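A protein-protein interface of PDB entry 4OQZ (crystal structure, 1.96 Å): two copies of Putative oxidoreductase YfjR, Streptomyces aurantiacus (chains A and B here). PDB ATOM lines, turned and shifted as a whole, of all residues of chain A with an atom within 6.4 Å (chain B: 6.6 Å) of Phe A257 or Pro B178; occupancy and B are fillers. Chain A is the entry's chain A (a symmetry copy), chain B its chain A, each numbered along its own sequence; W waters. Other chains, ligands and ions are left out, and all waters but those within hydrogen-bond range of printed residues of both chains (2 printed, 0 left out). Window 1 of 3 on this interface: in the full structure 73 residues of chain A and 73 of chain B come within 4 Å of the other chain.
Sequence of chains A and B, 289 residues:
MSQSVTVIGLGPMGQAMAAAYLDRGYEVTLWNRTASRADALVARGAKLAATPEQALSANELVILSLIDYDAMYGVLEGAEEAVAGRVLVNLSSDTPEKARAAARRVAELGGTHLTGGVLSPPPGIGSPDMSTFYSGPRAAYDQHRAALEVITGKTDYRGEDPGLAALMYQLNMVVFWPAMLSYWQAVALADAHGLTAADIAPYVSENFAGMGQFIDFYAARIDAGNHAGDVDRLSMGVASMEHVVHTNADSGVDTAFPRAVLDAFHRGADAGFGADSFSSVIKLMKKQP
Hydrophobic or aromatic side chains of chain B within 4 Å of the printed part of chain A: Val B174, Val B175, Trp B177, Pro B178, Leu B181, Phe B257, Ala B260, Val B261, Ala B264 and Met B285. Hydrophobic or aromatic side chains of chain A within 4 Å of the printed part of chain B: Pro A178, Leu A181, Met A241, Phe A257, Ala A260, Val A261 and Phe A265. Among the printed residues, 15 pairs touch across the chains. Among the printed residues, no Asp or Glu carboxylate lies within 4 Å of a Lys or Arg side-chain nitrogen of the other chain.
NE2 of Gln A185 lies within hydrogen-bond range of O of Asp A254, at 2.8 Å. OG of Ser A182 sits at hydrogen-bond distance from O of Ala A179, at 2.8 Å.
The backbone carbonyl oxygen of Met B285 sits at hydrogen-bond distance from the backbone NH of Asp A254 (2.9 Å).
Pro B178 touches just these residues of chain A: Phe A257 (3.5 Å) and Val A261 (3.7 Å). Of the printed residues of chain A, Val B175 touches Ser A182 (3.8 Å). Of the printed residues of chain A, Trp B177 touches Met A241, Val A261 and Phe A265. Met B173 touches none of the printed residues of chain A. The nearest printed residue of chain B that does not touch Phe A257 is Phe B257 (4.01 Å). The nearest residue of chain A that does not touch Pro B178 is Ser A182 (4.3 Å). The nearest printed residue of chain B that does not touch Asp A254 is Ala B264 (6.8 Å).
Val B261 touches Pro A178. Leu A181 touches Val B261 (CD2 to CA, 3.99 Å). Leu A181 touches Met B285. Ser A182 touches Val B174. Trp B177 touches Met A241. Ala B260 touches Ala A260. Val A261 touches Trp B177. CG2 of Val A261 touches CG of Pro B178, at 3.7 Å. CD2 of Leu B181 touches CA of Val A261, at 3.99 Å. CE2 of Phe A265 touches CE3 of Trp B177, at 3.5 Å.
Pro A178 touches Phe B257, and with the chains exchanged Phe A257 touches Pro B178. Pro A178 touches Val B261, and with the chains exchanged Val A261 touches Pro B178. Leu A181 touches Val B261, and with the chains exchanged Val A261 touches Leu B181. Ala B260 touches its own counterpart, Ala A260. Positions printed for both chains: 178, 179, 181, 182, 183, 257, 260 and 261. Of the 15 pairs that touch across the chains among the printed residues, 7 have their exchanged pair printed and touching as well.
Water W1 lies within hydrogen-bond range of the backbone carbonyl oxygen of Val B175 (2.6 Å), the side-chain hydroxyl of Ser A182 (2.7 Å) and the backbone NH of Ala B179 (3.1 Å). Water W2 lies within hydrogen-bond range of OG of Ser B182 and N of Ala A179.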
ATOM      1  N   PRO A 178      24.466  -9.045   6.059  1.00  0.00           N
ATOM      2  CA  PRO A 178      24.535  -7.654   6.538  1.00  0.00           C
ATOM      3  C   PRO A 178      25.714  -6.896   5.989  1.00  0.00           C
ATOM      4  O   PRO A 178      25.573  -5.705   5.778  1.00  0.00           O
ATOM      5  CB  PRO A 178      24.667  -7.806   8.067  1.00  0.00           C
ATOM      6  CG  PRO A 178      24.167  -9.173   8.364  1.00  0.00           C
ATOM      7  CD  PRO A 178      24.611  -9.986   7.194  1.00  0.00           C
ATOM      8  N   ALA A 179      26.891  -7.540   5.809  1.00  0.00           N
ATOM      9  CA  ALA A 179      28.039  -6.852   5.225  1.00  0.00           C
ATOM     10  C   ALA A 179      27.673  -6.344   3.841  1.00  0.00           C
ATOM     11  O   ALA A 179      27.819  -5.151   3.542  1.00  0.00           O
ATOM     12  CB  ALA A 179      29.222  -7.791   5.135  1.00  0.00           C
ATOM     13  N   LEU A 181      24.605  -5.873   2.658  1.00  0.00           N
ATOM     14  CA  LEU A 181      23.538  -4.907   2.847  1.00  0.00           C
ATOM     15  C   LEU A 181      24.071  -3.541   3.281  1.00  0.00           C
ATOM     16  O   LEU A 181      23.524  -2.524   2.831  1.00  0.00           O
ATOM     17  CB  LEU A 181      22.481  -5.425   3.824  1.00  0.00           C
ATOM     18  CG  LEU A 181      21.201  -4.547   3.986  1.00  0.00           C
ATOM     19  CD1 LEU A 181      20.511  -4.296   2.628  1.00  0.00           C
ATOM     20  CD2 LEU A 181      20.232  -5.179   4.929  1.00  0.00           C
ATOM     21  N   SER A 182      25.170  -3.513   4.113  1.00  0.00           N
ATOM     22  CA  SER A 182      25.794  -2.259   4.546  1.00  0.00           C
ATOM     23  C   SER A 182      26.444  -1.607   3.336  1.00  0.00           C
ATOM     24  O   SER A 182      26.445  -0.379   3.223  1.00  0.00           O
ATOM     25  CB  SER A 182      26.755  -2.470   5.706  1.00  0.00           C
ATOM     26  OG  SER A 182      28.010  -2.976   5.263  1.00  0.00           O
ATOM     27  N   TYR A 183      26.971  -2.430   2.426  1.00  0.00           N
ATOM     28  CA  TYR A 183      27.497  -1.931   1.147  1.00  0.00           C
ATOM     29  C   TYR A 183      26.351  -1.362   0.302  1.00  0.00           C
ATOM     30  O   TYR A 183      26.503  -0.277  -0.250  1.00  0.00           O
ATOM     31  CB  TYR A 183      28.345  -2.976   0.385  1.00  0.00           C
ATOM     32  CG  TYR A 183      28.949  -2.429  -0.899  1.00  0.00           C
ATOM     33  CD1 TYR A 183      29.650  -1.225  -0.904  1.00  0.00           C
ATOM     34  CD2 TYR A 183      28.784  -3.094  -2.109  1.00  0.00           C
ATOM     35  CE1 TYR A 183      30.218  -0.721  -2.067  1.00  0.00           C
ATOM     36  CE2 TYR A 183      29.300  -2.568  -3.300  1.00  0.00           C
ATOM     37  CZ  TYR A 183      30.003  -1.370  -3.274  1.00  0.00           C
ATOM     38  OH  TYR A 183      30.539  -0.832  -4.411  1.00  0.00           O
ATOM     39  N   GLN A 185      23.688  -0.030   1.445  1.00  0.00           N
ATOM     40  CA  GLN A 185      23.410   1.224   2.140  1.00  0.00           C
ATOM     41  C   GLN A 185      24.430   2.352   1.817  1.00  0.00           C
ATOM     42  O   GLN A 185      24.034   3.512   1.680  1.00  0.00           O
ATOM     43  CB  GLN A 185      23.327   0.987   3.650  1.00  0.00           C
ATOM     44  CG  GLN A 185      22.883   2.212   4.422  1.00  0.00           C
ATOM     45  CD  GLN A 185      21.409   2.481   4.328  1.00  0.00           C
ATOM     46  OE1 GLN A 185      20.576   1.564   4.346  1.00  0.00           O
ATOM     47  NE2 GLN A 185      21.056   3.750   4.230  1.00  0.00           N
ATOM     48  N   MET A 241      26.130   6.265  15.412  1.00  0.00           N
ATOM     49  CA  MET A 241      25.028   5.707  14.645  1.00  0.00           C
ATOM     50  C   MET A 241      23.892   6.717  14.408  1.00  0.00           C
ATOM     51  O   MET A 241      23.252   6.657  13.355  1.00  0.00           O
ATOM     52  CB  MET A 241      24.527   4.395  15.252  1.00  0.00           C
ATOM     53  CG  MET A 241      25.257   3.183  14.734  1.00  0.00           C
ATOM     54  SD  MET A 241      25.575   3.160  12.942  1.00  0.00           S
ATOM     55  CE  MET A 241      23.853   3.108  12.258  1.00  0.00           C
ATOM     56  N   ASP A 254      16.999   6.009   2.465  1.00  0.00           N
ATOM     57  CA  ASP A 254      16.317   5.136   3.425  1.00  0.00           C
ATOM     58  C   ASP A 254      17.190   4.861   4.674  1.00  0.00           C
ATOM     59  O   ASP A 254      18.356   4.487   4.546  1.00  0.00           O
ATOM     60  CB  ASP A 254      15.921   3.826   2.715  1.00  0.00           C
ATOM     61  CG  ASP A 254      15.013   2.902   3.496  1.00  0.00           C
ATOM     62  OD1 ASP A 254      13.807   3.239   3.649  1.00  0.00           O
ATOM     63  OD2 ASP A 254      15.480   1.801   3.886  1.00  0.00           O
ATOM     64  N   THR A 255      16.622   5.075   5.876  1.00  0.00           N
ATOM     65  CA  THR A 255      17.293   4.876   7.169  1.00  0.00           C
ATOM     66  C   THR A 255      16.922   3.569   7.887  1.00  0.00           C
ATOM     67  O   THR A 255      17.318   3.414   9.041  1.00  0.00           O
ATOM     68  CB  THR A 255      17.086   6.087   8.111  1.00  0.00           C
ATOM     69  OG1 THR A 255      15.690   6.294   8.369  1.00  0.00           O
ATOM     70  CG2 THR A 255      17.733   7.351   7.602  1.00  0.00           C
ATOM     71  N   ALA A 256      16.215   2.621   7.221  1.00  0.00           N
ATOM     72  CA  ALA A 256      15.797   1.344   7.832  1.00  0.00           C
ATOM     73  C   ALA A 256      16.944   0.472   8.373  1.00  0.00           C
ATOM     74  O   ALA A 256      16.900   0.088   9.542  1.00  0.00           O
ATOM     75  CB  ALA A 256      14.885   0.550   6.895  1.00  0.00           C
ATOM     76  N   PHE A 257      17.964   0.175   7.549  1.00  0.00           N
ATOM     77  CA  PHE A 257      19.141  -0.605   7.986  1.00  0.00           C
ATOM     78  C   PHE A 257      19.964   0.146   9.049  1.00  0.00           C
ATOM     79  O   PHE A 257      20.188  -0.445  10.102  1.00  0.00           O
ATOM     80  CB  PHE A 257      19.997  -1.067   6.801  1.00  0.00           C
ATOM     81  CG  PHE A 257      21.217  -1.871   7.187  1.00  0.00           C
ATOM     82  CD1 PHE A 257      21.089  -3.076   7.866  1.00  0.00           C
ATOM     83  CD2 PHE A 257      22.487  -1.448   6.829  1.00  0.00           C
ATOM     84  CE1 PHE A 257      22.221  -3.823   8.221  1.00  0.00           C
ATOM     85  CE2 PHE A 257      23.611  -2.191   7.186  1.00  0.00           C
ATOM     86  CZ  PHE A 257      23.471  -3.388   7.851  1.00  0.00           C
ATOM     87  N   PRO A 258      20.331   1.453   8.882  1.00  0.00           N
ATOM     88  CA  PRO A 258      21.070   2.138   9.953  1.00  0.00           C
ATOM     89  C   PRO A 258      20.268   2.332  11.235  1.00  0.00           C
ATOM     90  O   PRO A 258      20.875   2.358  12.292  1.00  0.00           O
ATOM     91  CB  PRO A 258      21.436   3.490   9.330  1.00  0.00           C
ATOM     92  CG  PRO A 258      21.330   3.288   7.861  1.00  0.00           C
ATOM     93  CD  PRO A 258      20.173   2.352   7.715  1.00  0.00           C
ATOM     94  N   ARG A 259      18.920   2.503  11.179  1.00  0.00           N
ATOM     95  CA  ARG A 259      18.227   2.648  12.452  1.00  0.00           C
ATOM     96  C   ARG A 259      18.167   1.336  13.208  1.00  0.00           C
ATOM     97  O   ARG A 259      18.344   1.336  14.412  1.00  0.00           O
ATOM     98  CB  ARG A 259      16.886   3.429  12.398  1.00  0.00           C
ATOM     99  CG  ARG A 259      15.780   2.862  11.521  1.00  0.00           C
ATOM    100  CD  ARG A 259      14.502   3.711  11.585  1.00  0.00           C
ATOM    101  NE  ARG A 259      14.655   5.057  11.014  1.00  0.00           N
ATOM    102  CZ  ARG A 259      14.940   6.158  11.712  1.00  0.00           C
ATOM    103  NH1 ARG A 259      15.047   7.330  11.101  1.00  0.00           N
ATOM    104  NH2 ARG A 259      15.099   6.096  13.031  1.00  0.00           N
ATOM    105  N   ALA A 260      18.064   0.214  12.493  1.00  0.00           N
ATOM    106  CA  ALA A 260      18.092  -1.136  13.075  1.00  0.00           C
ATOM    107  C   ALA A 260      19.373  -1.356  13.891  1.00  0.00           C
ATOM    108  O   ALA A 260      19.311  -1.917  14.991  1.00  0.00           O
ATOM    109  CB  ALA A 260      18.009  -2.166  11.966  1.00  0.00           C
ATOM    110  N   VAL A 261      20.526  -0.856  13.373  1.00  0.00           N
ATOM    111  CA  VAL A 261      21.843  -0.907  14.037  1.00  0.00           C
ATOM    112  C   VAL A 261      21.821   0.045  15.238  1.00  0.00           C
ATOM    113  O   VAL A 261      22.207  -0.357  16.333  1.00  0.00           O
ATOM    114  CB  VAL A 261      22.998  -0.597  13.040  1.00  0.00           C
ATOM    115  CG1 VAL A 261      24.349  -0.453  13.748  1.00  0.00           C
ATOM    116  CG2 VAL A 261      23.059  -1.639  11.934  1.00  0.00           C
ATOM    117  N   LEU A 262      21.355   1.301  15.036  1.00  0.00           N
ATOM    118  CA  LEU A 262      21.206   2.307  16.101  1.00  0.00           C
ATOM    119  C   LEU A 262      20.323   1.758  17.217  1.00  0.00           C
ATOM    120  O   LEU A 262      20.667   1.926  18.380  1.00  0.00           O
ATOM    121  CB  LEU A 262      20.586   3.613  15.538  1.00  0.00           C
ATOM    122  CG  LEU A 262      20.062   4.691  16.520  1.00  0.00           C
ATOM    123  CD1 LEU A 262      21.192   5.342  17.327  1.00  0.00           C
ATOM    124  CD2 LEU A 262      19.325   5.761  15.776  1.00  0.00           C
ATOM    125  N   PHE A 265      22.160  -0.433  19.622  1.00  0.00           N
ATOM    126  CA  PHE A 265      23.077   0.350  20.446  1.00  0.00           C
ATOM    127  C   PHE A 265      22.338   1.147  21.506  1.00  0.00           C
ATOM    128  O   PHE A 265      22.778   1.134  22.655  1.00  0.00           O
ATOM    129  CB  PHE A 265      23.954   1.267  19.592  1.00  0.00           C
ATOM    130  CG  PHE A 265      24.989   0.569  18.733  1.00  0.00           C
ATOM    131  CD1 PHE A 265      25.292  -0.776  18.926  1.00  0.00           C
ATOM    132  CD2 PHE A 265      25.698   1.271  17.765  1.00  0.00           C
ATOM    133  CE1 PHE A 265      26.255  -1.417  18.131  1.00  0.00           C
ATOM    134  CE2 PHE A 265      26.674   0.636  16.989  1.00  0.00           C
ATOM    135  CZ  PHE A 265      26.939  -0.703  17.173  1.00  0.00           C
ATOM    136  N   ASN B 172      32.182   5.129   6.063  1.00  0.00           N
ATOM    137  CA  ASN B 172      32.968   4.183   6.832  1.00  0.00           C
ATOM    138  C   ASN B 172      32.146   3.579   8.005  1.00  0.00           C
ATOM    139  O   ASN B 172      32.182   2.368   8.224  1.00  0.00           O
ATOM    140  CB  ASN B 172      34.224   4.880   7.392  1.00  0.00           C
ATOM    141  CG  ASN B 172      35.186   3.931   8.037  1.00  0.00           C
ATOM    142  OD1 ASN B 172      35.064   3.560   9.212  1.00  0.00           O
ATOM    143  ND2 ASN B 172      36.147   3.484   7.261  1.00  0.00           N
ATOM    144  N   MET B 173      31.449   4.429   8.770  1.00  0.00           N
ATOM    145  CA  MET B 173      30.683   4.018   9.953  1.00  0.00           C
ATOM    146  C   MET B 173      29.446   3.190   9.567  1.00  0.00           C
ATOM    147  O   MET B 173      29.059   2.298  10.319  1.00  0.00           O
ATOM    148  CB  MET B 173      30.319   5.238  10.818  1.00  0.00           C
ATOM    149  CG  MET B 173      31.519   6.048  11.327  1.00  0.00           C
ATOM    150  SD  MET B 173      33.082   5.180  11.737  1.00  0.00           S
ATOM    151  CE  MET B 173      32.602   4.284  13.089  1.00  0.00           C
ATOM    152  N   VAL B 174      28.880   3.444   8.360  1.00  0.00           N
ATOM    153  CA  VAL B 174      27.776   2.693   7.740  1.00  0.00           C
ATOM    154  C   VAL B 174      28.134   1.209   7.640  1.00  0.00           C
ATOM    155  O   VAL B 174      27.284   0.353   7.741  1.00  0.00           O
ATOM    156  CB  VAL B 174      27.416   3.295   6.353  1.00  0.00           C
ATOM    157  CG1 VAL B 174      26.921   2.247   5.367  1.00  0.00           C
ATOM    158  CG2 VAL B 174      26.394   4.408   6.490  1.00  0.00           C
ATOM    159  N   VAL B 175      29.391   0.933   7.384  1.00  0.00           N
ATOM    160  CA  VAL B 175      29.933  -0.385   7.207  1.00  0.00           C
ATOM    161  C   VAL B 175      30.451  -0.951   8.543  1.00  0.00           C
ATOM    162  O   VAL B 175      30.153  -2.099   8.870  1.00  0.00           O
ATOM    163  CB  VAL B 175      31.050  -0.297   6.142  1.00  0.00           C
ATOM    164  CG1 VAL B 175      31.929  -1.539   6.156  1.00  0.00           C
ATOM    165  CG2 VAL B 175      30.464  -0.055   4.756  1.00  0.00           C
ATOM    166  N   PHE B 176      31.265  -0.182   9.277  1.00  0.00           N
ATOM    167  CA  PHE B 176      31.891  -0.624  10.532  1.00  0.00           C
ATOM    168  C   PHE B 176      30.911  -1.092  11.618  1.00  0.00           C
ATOM    169  O   PHE B 176      31.012  -2.212  12.112  1.00  0.00           O
ATOM    170  CB  PHE B 176      32.760   0.502  11.101  1.00  0.00           C
ATOM    171  CG  PHE B 176      33.432   0.127  12.401  1.00  0.00           C
ATOM    172  CD1 PHE B 176      34.563  -0.687  12.410  1.00  0.00           C
ATOM    173  CD2 PHE B 176      32.918   0.561  13.621  1.00  0.00           C
ATOM    174  CE1 PHE B 176      35.163  -1.061  13.610  1.00  0.00           C
ATOM    175  CE2 PHE B 176      33.521   0.180  14.819  1.00  0.00           C
ATOM    176  CZ  PHE B 176      34.637  -0.628  14.801  1.00  0.00           C
ATOM    177  N   TRP B 177      29.995  -0.227  12.002  1.00  0.00           N
ATOM    178  CA  TRP B 177      29.032  -0.539  13.084  1.00  0.00           C
ATOM    179  C   TRP B 177      28.228  -1.796  12.825  1.00  0.00           C
ATOM    180  O   TRP B 177      28.302  -2.672  13.673  1.00  0.00           O
ATOM    181  CB  TRP B 177      28.157   0.645  13.414  1.00  0.00           C
ATOM    182  CG  TRP B 177      28.881   1.841  13.944  1.00  0.00           C
ATOM    183  CD1 TRP B 177      28.790   3.119  13.471  1.00  0.00           C
ATOM    184  CD2 TRP B 177      29.692   1.908  15.129  1.00  0.00           C
ATOM    185  NE1 TRP B 177      29.487   3.977  14.286  1.00  0.00           N
ATOM    186  CE2 TRP B 177      30.038   3.266  15.320  1.00  0.00           C
ATOM    187  CE3 TRP B 177      30.053   0.977  16.122  1.00  0.00           C
ATOM    188  CZ2 TRP B 177      30.849   3.692  16.384  1.00  0.00           C
ATOM    189  CZ3 TRP B 177      30.852   1.398  17.178  1.00  0.00           C
ATOM    190  CH2 TRP B 177      31.266   2.734  17.286  1.00  0.00           C
ATOM    191  N   PRO B 178      27.597  -1.984  11.622  1.00  0.00           N
ATOM    192  CA  PRO B 178      26.903  -3.251  11.337  1.00  0.00           C
ATOM    193  C   PRO B 178      27.836  -4.427  11.227  1.00  0.00           C
ATOM    194  O   PRO B 178      27.430  -5.510  11.609  1.00  0.00           O
ATOM    195  CB  PRO B 178      26.217  -2.990   9.981  1.00  0.00           C
ATOM    196  CG  PRO B 178      26.149  -1.510   9.861  1.00  0.00           C
ATOM    197  CD  PRO B 178      27.412  -1.035  10.499  1.00  0.00           C
ATOM    198  N   ALA B 179      29.054  -4.257  10.661  1.00  0.00           N
ATOM    199  CA  ALA B 179      30.007  -5.361  10.589  1.00  0.00           C
ATOM    200  C   ALA B 179      30.312  -5.857  11.992  1.00  0.00           C
ATOM    201  O   ALA B 179      30.172  -7.051  12.289  1.00  0.00           O
ATOM    202  CB  ALA B 179      31.283  -4.908   9.913  1.00  0.00           C
ATOM    203  N   MET B 180      30.601  -4.919  12.910  1.00  0.00           N
ATOM    204  CA  MET B 180      30.868  -5.285  14.304  1.00  0.00           C
ATOM    205  C   MET B 180      29.673  -5.880  15.003  1.00  0.00           C
ATOM    206  O   MET B 180      29.849  -6.852  15.749  1.00  0.00           O
ATOM    207  CB  MET B 180      31.462  -4.128  15.111  1.00  0.00           C
ATOM    208  CG  MET B 180      32.892  -3.743  14.699  1.00  0.00           C
ATOM    209  SD  MET B 180      34.111  -5.099  14.591  1.00  0.00           S
ATOM    210  CE  MET B 180      34.151  -5.640  16.325  1.00  0.00           C
ATOM    211  N   LEU B 181      28.466  -5.355  14.708  1.00  0.00           N
ATOM    212  CA  LEU B 181      27.215  -5.863  15.242  1.00  0.00           C
ATOM    213  C   LEU B 181      26.906  -7.273  14.738  1.00  0.00           C
ATOM    214  O   LEU B 181      26.384  -8.078  15.522  1.00  0.00           O
ATOM    215  CB  LEU B 181      26.056  -4.907  14.956  1.00  0.00           C
ATOM    216  CG  LEU B 181      24.689  -5.261  15.620  1.00  0.00           C
ATOM    217  CD1 LEU B 181      24.822  -5.401  17.152  1.00  0.00           C
ATOM    218  CD2 LEU B 181      23.655  -4.233  15.302  1.00  0.00           C
ATOM    219  N   SER B 182      27.275  -7.591  13.448  1.00  0.00           N
ATOM    220  CA  SER B 182      27.075  -8.930  12.883  1.00  0.00           C
ATOM    221  C   SER B 182      28.007  -9.894  13.600  1.00  0.00           C
ATOM    222  O   SER B 182      27.642 -11.050  13.826  1.00  0.00           O
ATOM    223  CB  SER B 182      27.242  -8.941  11.371  1.00  0.00           C
ATOM    224  OG  SER B 182      28.615  -8.956  10.994  1.00  0.00           O
ATOM    225  N   TYR B 183      29.193  -9.410  13.976  1.00  0.00           N
ATOM    226  CA  TYR B 183      30.121 -10.197  14.801  1.00  0.00           C
ATOM    227  C   TYR B 183      29.515 -10.419  16.192  1.00  0.00           C
ATOM    228  O   TYR B 183      29.557 -11.542  16.684  1.00  0.00           O
ATOM    229  CB  TYR B 183      31.547  -9.601  14.854  1.00  0.00           C
ATOM    230  CG  TYR B 183      32.521 -10.461  15.645  1.00  0.00           C
ATOM    231  CD1 TYR B 183      32.637 -11.827  15.395  1.00  0.00           C
ATOM    232  CD2 TYR B 183      33.291  -9.916  16.666  1.00  0.00           C
ATOM    233  CE1 TYR B 183      33.531 -12.620  16.102  1.00  0.00           C
ATOM    234  CE2 TYR B 183      34.154 -10.715  17.428  1.00  0.00           C
ATOM    235  CZ  TYR B 183      34.256 -12.072  17.150  1.00  0.00           C
ATOM    236  OH  TYR B 183      35.101 -12.883  17.856  1.00  0.00           O
ATOM    237  N   PHE B 208      35.334 -11.356   6.178  1.00  0.00           N
ATOM    238  CA  PHE B 208      35.483  -9.933   5.890  1.00  0.00           C
ATOM    239  C   PHE B 208      36.604  -9.663   4.912  1.00  0.00           C
ATOM    240  O   PHE B 208      36.453  -8.794   4.052  1.00  0.00           O
ATOM    241  CB  PHE B 208      35.734  -9.147   7.179  1.00  0.00           C
ATOM    242  CG  PHE B 208      34.481  -8.957   8.010  1.00  0.00           C
ATOM    243  CD1 PHE B 208      33.324  -8.438   7.446  1.00  0.00           C
ATOM    244  CD2 PHE B 208      34.478  -9.245   9.361  1.00  0.00           C
ATOM    245  CE1 PHE B 208      32.167  -8.240   8.220  1.00  0.00           C
ATOM    246  CE2 PHE B 208      33.311  -9.060  10.130  1.00  0.00           C
ATOM    247  CZ  PHE B 208      32.175  -8.555   9.549  1.00  0.00           C
ATOM    248  N   PHE B 257      18.630  -8.144  14.956  1.00  0.00           N
ATOM    249  CA  PHE B 257      19.555  -7.780  13.864  1.00  0.00           C
ATOM    250  C   PHE B 257      19.336  -8.650  12.613  1.00  0.00           C
ATOM    251  O   PHE B 257      19.134  -8.064  11.553  1.00  0.00           O
ATOM    252  CB  PHE B 257      21.017  -7.777  14.326  1.00  0.00           C
ATOM    253  CG  PHE B 257      22.011  -7.410  13.249  1.00  0.00           C
ATOM    254  CD1 PHE B 257      21.961  -6.170  12.626  1.00  0.00           C
ATOM    255  CD2 PHE B 257      23.026  -8.286  12.895  1.00  0.00           C
ATOM    256  CE1 PHE B 257      22.887  -5.831  11.629  1.00  0.00           C
ATOM    257  CE2 PHE B 257      23.943  -7.947  11.901  1.00  0.00           C
ATOM    258  CZ  PHE B 257      23.888  -6.711  11.296  1.00  0.00           C
ATOM    259  N   ALA B 260      15.977  -7.678  10.808  1.00  0.00           N
ATOM    260  CA  ALA B 260      16.149  -6.368  10.164  1.00  0.00           C
ATOM    261  C   ALA B 260      16.752  -6.521   8.761  1.00  0.00           C
ATOM    262  O   ALA B 260      16.296  -5.857   7.823  1.00  0.00           O
ATOM    263  CB  ALA B 260      17.054  -5.501  11.017  1.00  0.00           C
ATOM    264  N   VAL B 261      17.738  -7.443   8.612  1.00  0.00           N
ATOM    265  CA  VAL B 261      18.392  -7.783   7.333  1.00  0.00           C
ATOM    266  C   VAL B 261      17.385  -8.531   6.453  1.00  0.00           C
ATOM    267  O   VAL B 261      17.217  -8.172   5.290  1.00  0.00           O
ATOM    268  CB  VAL B 261      19.709  -8.582   7.558  1.00  0.00           C
ATOM    269  CG1 VAL B 261      20.297  -9.109   6.246  1.00  0.00           C
ATOM    270  CG2 VAL B 261      20.726  -7.753   8.328  1.00  0.00           C
ATOM    271  N   ALA B 264      14.695  -6.247   4.896  1.00  0.00           N
ATOM    272  CA  ALA B 264      15.163  -5.536   3.703  1.00  0.00           C
ATOM    273  C   ALA B 264      15.147  -6.412   2.446  1.00  0.00           C
ATOM    274  O   ALA B 264      14.858  -5.896   1.372  1.00  0.00           O
ATOM    275  CB  ALA B 264      16.545  -4.961   3.929  1.00  0.00           C
ATOM    276  N   MET B 285      16.442   1.940  -1.632  1.00  0.00           N
ATOM    277  CA  MET B 285      17.157   2.729  -0.618  1.00  0.00           C
ATOM    278  C   MET B 285      17.498   4.146  -1.051  1.00  0.00           C
ATOM    279  O   MET B 285      17.484   5.039  -0.208  1.00  0.00           O
ATOM    280  CB  MET B 285      18.416   2.018  -0.099  1.00  0.00           C
ATOM    281  CG  MET B 285      18.139   0.741   0.620  1.00  0.00           C
ATOM    282  SD  MET B 285      19.625  -0.257   0.518  1.00  0.00           S
ATOM    283  CE  MET B 285      18.929  -1.800   0.236  1.00  0.00           C
HETATM  284  O   HOH W   1      28.996  -4.027   7.540  1.00  0.00           O
HETATM  285  O   HOH W   2      28.481  -8.073   8.452  1.00  0.00           O
